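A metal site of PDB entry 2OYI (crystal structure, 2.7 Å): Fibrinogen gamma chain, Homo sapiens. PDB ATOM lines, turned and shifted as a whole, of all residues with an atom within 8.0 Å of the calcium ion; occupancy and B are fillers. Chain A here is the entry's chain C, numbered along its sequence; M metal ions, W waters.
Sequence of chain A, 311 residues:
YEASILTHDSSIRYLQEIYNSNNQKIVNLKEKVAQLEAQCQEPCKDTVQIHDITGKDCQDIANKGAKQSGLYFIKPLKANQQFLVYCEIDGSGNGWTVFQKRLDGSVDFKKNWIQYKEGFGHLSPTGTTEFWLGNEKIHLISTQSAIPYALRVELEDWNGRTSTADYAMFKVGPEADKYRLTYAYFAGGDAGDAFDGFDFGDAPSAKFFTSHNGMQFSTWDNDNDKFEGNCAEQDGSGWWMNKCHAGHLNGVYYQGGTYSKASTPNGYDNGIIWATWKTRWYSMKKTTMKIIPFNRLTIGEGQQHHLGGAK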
ATOM      1  N   SER A 218      -8.489  31.736 -19.842  1.00  0.00           N
ATOM      2  CA  SER A 218      -8.837  30.328 -19.967  1.00  0.00           C
ATOM      3  C   SER A 218      -7.819  29.429 -19.272  1.00  0.00           C
ATOM      4  O   SER A 218      -6.630  29.703 -19.309  1.00  0.00           O
ATOM      5  CB  SER A 218      -8.927  29.932 -21.447  1.00  0.00           C
ATOM      6  OG  SER A 218      -9.805  30.769 -22.168  1.00  0.00           O
ATOM      7  N   ASN A 222     -11.244  25.311 -16.995  1.00  0.00           N
ATOM      8  CA  ASN A 222     -12.222  26.369 -17.242  1.00  0.00           C
ATOM      9  C   ASN A 222     -11.942  26.966 -18.616  1.00  0.00           C
ATOM     10  O   ASN A 222     -11.231  27.973 -18.739  1.00  0.00           O
ATOM     11  CB  ASN A 222     -12.112  27.430 -16.134  1.00  0.00           C
ATOM     12  CG  ASN A 222     -13.292  28.402 -16.124  1.00  0.00           C
ATOM     13  OD1 ASN A 222     -13.522  29.097 -15.129  1.00  0.00           O
ATOM     14  ND2 ASN A 222     -14.021  28.473 -17.229  1.00  0.00           N
ATOM     15  N   ASP A 223     -12.502  26.326 -19.641  1.00  0.00           N
ATOM     16  CA  ASP A 223     -12.341  26.716 -21.041  1.00  0.00           C
ATOM     17  C   ASP A 223     -13.270  27.851 -21.482  1.00  0.00           C
ATOM     18  O   ASP A 223     -14.483  27.737 -21.383  1.00  0.00           O
ATOM     19  CB  ASP A 223     -12.600  25.478 -21.923  1.00  0.00           C
ATOM     20  CG  ASP A 223     -12.307  25.728 -23.404  1.00  0.00           C
ATOM     21  OD1 ASP A 223     -12.724  26.783 -23.929  1.00  0.00           O
ATOM     22  OD2 ASP A 223     -11.666  24.856 -24.035  1.00  0.00           O
ATOM     23  N   ASN A 224     -12.683  28.946 -21.947  1.00  0.00           N
ATOM     24  CA  ASN A 224     -13.468  30.093 -22.423  1.00  0.00           C
ATOM     25  C   ASN A 224     -12.841  30.642 -23.685  1.00  0.00           C
ATOM     26  O   ASN A 224     -12.939  31.835 -23.960  1.00  0.00           O
ATOM     27  CB  ASN A 224     -13.512  31.211 -21.369  1.00  0.00           C
ATOM     28  CG  ASN A 224     -13.896  30.697 -20.002  1.00  0.00           C
ATOM     29  OD1 ASN A 224     -13.034  30.386 -19.177  1.00  0.00           O
ATOM     30  ND2 ASN A 224     -15.194  30.613 -19.755  1.00  0.00           N
ATOM     31  N   ASP A 225     -12.196  29.778 -24.443  1.00  0.00           N
ATOM     32  CA  ASP A 225     -11.553  30.182 -25.685  1.00  0.00           C
ATOM     33  C   ASP A 225     -12.488  29.999 -26.866  1.00  0.00           C
ATOM     34  O   ASP A 225     -13.564  29.399 -26.739  1.00  0.00           O
ATOM     35  CB  ASP A 225     -10.283  29.364 -25.917  1.00  0.00           C
ATOM     36  CG  ASP A 225     -10.566  27.871 -26.050  1.00  0.00           C
ATOM     37  OD1 ASP A 225     -11.611  27.511 -26.648  1.00  0.00           O
ATOM     38  OD2 ASP A 225      -9.744  27.066 -25.556  1.00  0.00           O
ATOM     39  N   LYS A 226     -12.063  30.494 -28.019  1.00  0.00           N
ATOM     40  CA  LYS A 226     -12.835  30.395 -29.257  1.00  0.00           C
ATOM     41  C   LYS A 226     -12.380  29.195 -30.082  1.00  0.00           C
ATOM     42  O   LYS A 226     -12.072  29.321 -31.270  1.00  0.00           O
ATOM     43  CB  LYS A 226     -12.666  31.684 -30.062  1.00  0.00           C
ATOM     44  CG  LYS A 226     -12.877  32.963 -29.261  1.00  0.00           C
ATOM     45  CD  LYS A 226     -14.227  33.001 -28.550  1.00  0.00           C
ATOM     46  CE  LYS A 226     -14.449  34.352 -27.871  1.00  0.00           C
ATOM     47  NZ  LYS A 226     -15.653  34.414 -26.987  1.00  0.00           N
ATOM     48  N   PHE A 227     -12.348  28.027 -29.453  1.00  0.00           N
ATOM     49  CA  PHE A 227     -11.907  26.792 -30.105  1.00  0.00           C
ATOM     50  C   PHE A 227     -12.712  25.643 -29.490  1.00  0.00           C
ATOM     51  O   PHE A 227     -12.856  25.554 -28.280  1.00  0.00           O
ATOM     52  CB  PHE A 227     -10.396  26.621 -29.858  1.00  0.00           C
ATOM     53  CG  PHE A 227      -9.821  25.323 -30.369  1.00  0.00           C
ATOM     54  CD1 PHE A 227     -10.104  24.869 -31.663  1.00  0.00           C
ATOM     55  CD2 PHE A 227      -8.979  24.558 -29.561  1.00  0.00           C
ATOM     56  CE1 PHE A 227      -9.554  23.671 -32.134  1.00  0.00           C
ATOM     57  CE2 PHE A 227      -8.414  23.361 -30.024  1.00  0.00           C
ATOM     58  CZ  PHE A 227      -8.702  22.918 -31.310  1.00  0.00           C
ATOM     59  N   GLU A 228     -13.255  24.775 -30.342  1.00  0.00           N
ATOM     60  CA  GLU A 228     -14.047  23.646 -29.863  1.00  0.00           C
ATOM     61  C   GLU A 228     -13.212  22.848 -28.871  1.00  0.00           C
ATOM     62  O   GLU A 228     -13.740  22.273 -27.912  1.00  0.00           O
ATOM     63  CB  GLU A 228     -14.438  22.740 -31.017  1.00  0.00           C
ATOM     64  CG  GLU A 228     -13.262  22.096 -31.704  1.00  0.00           C
ATOM     65  CD  GLU A 228     -13.679  21.099 -32.760  1.00  0.00           C
ATOM     66  OE1 GLU A 228     -12.792  20.368 -33.261  1.00  0.00           O
ATOM     67  OE2 GLU A 228     -14.892  21.064 -33.102  1.00  0.00           O
ATOM     68  N   GLY A 229     -11.906  22.820 -29.112  1.00  0.00           N
ATOM     69  CA  GLY A 229     -10.997  22.110 -28.232  1.00  0.00           C
ATOM     70  C   GLY A 229     -10.614  22.969 -27.044  1.00  0.00           C
ATOM     71  O   GLY A 229     -11.256  23.970 -26.754  1.00  0.00           O
ATOM     72  N   ASN A 230      -9.540  22.581 -26.359  1.00  0.00           N
ATOM     73  CA  ASN A 230      -9.116  23.323 -25.190  1.00  0.00           C
ATOM     74  C   ASN A 230      -7.684  23.841 -25.297  1.00  0.00           C
ATOM     75  O   ASN A 230      -6.733  23.126 -25.025  1.00  0.00           O
ATOM     76  CB  ASN A 230      -9.275  22.449 -23.949  1.00  0.00           C
ATOM     77  CG  ASN A 230      -9.184  23.227 -22.665  1.00  0.00           C
ATOM     78  OD1 ASN A 230      -9.571  22.733 -21.605  1.00  0.00           O
ATOM     79  ND2 ASN A 230      -8.666  24.463 -22.745  1.00  0.00           N
ATOM     80  N   CYS A 231      -7.555  25.100 -25.706  1.00  0.00           N
ATOM     81  CA  CYS A 231      -6.242  25.714 -25.832  1.00  0.00           C
ATOM     82  C   CYS A 231      -5.441  25.578 -24.547  1.00  0.00           C
ATOM     83  O   CYS A 231      -4.340  25.038 -24.549  1.00  0.00           O
ATOM     84  CB  CYS A 231      -6.397  27.197 -26.175  1.00  0.00           C
ATOM     85  SG  CYS A 231      -7.121  27.545 -27.799  1.00  0.00           S
ATOM     86  N   ALA A 232      -6.013  26.071 -23.452  1.00  0.00           N
ATOM     87  CA  ALA A 232      -5.357  26.020 -22.161  1.00  0.00           C
ATOM     88  C   ALA A 232      -4.835  24.640 -21.803  1.00  0.00           C
ATOM     89  O   ALA A 232      -3.725  24.499 -21.284  1.00  0.00           O
ATOM     90  CB  ALA A 232      -6.301  26.516 -21.078  1.00  0.00           C
ATOM     91  N   MET A 241      -6.784  32.810 -24.178  1.00  0.00           N
ATOM     92  CA  MET A 241      -6.797  32.034 -25.411  1.00  0.00           C
ATOM     93  C   MET A 241      -7.879  32.421 -26.403  1.00  0.00           C
ATOM     94  O   MET A 241      -8.961  32.874 -26.041  1.00  0.00           O
ATOM     95  CB  MET A 241      -6.943  30.537 -25.087  1.00  0.00           C
ATOM     96  CG  MET A 241      -5.800  29.977 -24.270  1.00  0.00           C
ATOM     97  SD  MET A 241      -4.266  30.045 -25.185  1.00  0.00           S
ATOM     98  CE  MET A 241      -3.271  28.873 -24.226  1.00  0.00           C
ATOM     99  N   ASN A 242      -7.535  32.232 -27.663  1.00  0.00           N
ATOM    100  CA  ASN A 242      -8.420  32.521 -28.789  1.00  0.00           C
ATOM    101  C   ASN A 242      -8.562  31.175 -29.518  1.00  0.00           C
ATOM    102  O   ASN A 242      -9.401  30.351 -29.147  1.00  0.00           O
ATOM    103  CB  ASN A 242      -7.778  33.587 -29.689  1.00  0.00           C
ATOM    104  CG  ASN A 242      -8.690  34.043 -30.820  1.00  0.00           C
ATOM    105  OD1 ASN A 242      -9.154  33.224 -31.619  1.00  0.00           O
ATOM    106  ND2 ASN A 242      -8.926  35.340 -30.902  1.00  0.00           N
ATOM    107  N   CYS A 244      -5.318  29.495 -31.367  1.00  0.00           N
ATOM    108  CA  CYS A 244      -5.274  29.666 -29.918  1.00  0.00           C
ATOM    109  C   CYS A 244      -4.556  30.946 -29.449  1.00  0.00           C
ATOM    110  O   CYS A 244      -5.094  31.705 -28.639  1.00  0.00           O
ATOM    111  CB  CYS A 244      -4.624  28.456 -29.251  1.00  0.00           C
ATOM    112  SG  CYS A 244      -5.673  26.969 -29.117  1.00  0.00           S
HETATM  113 CA    CA M   1     -12.865  25.737 -26.252  1.00  0.00          CA
HETATM  114  O   HOH W   1     -14.719  23.914 -26.059  1.00  0.00           O
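The side-chain carboxylate (OD2) of Asp 225 is in hydrogen-bond range of the backbone NH (N) of Cys 231 (2.9 Å). The backbone NH of Asp 225 sits at hydrogen-bond distance from the side-chain hydroxyl of Ser 218 (3.4 Å). The side-chain carboxylate (OD2) of Asp 223 lies close to the side-chain amide nitrogen (ND2) of Asn 230, 3.3 Å away. SG of Cys 231 is disulfide-bonded to SG of Cys 244.
Glu 228 touches the calcium ion (C to CA, 3.9 Å). Of the 15 residues printed, 5 come within 4 Å of the calcium ion. The nearest printed residue that does not touch the calcium ion is Asn 230 (4.6 Å).
The calcium ion is bound by O of Phe 227 (2.0 Å), OD1 of Asp 225 (2.2 Å), O of Gly 229 (2.4 Å), OD1 of Asp 223 (2.6 Å), water W1 (2.6 Å) and OD2 of Asp 223 (2.7 Å).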
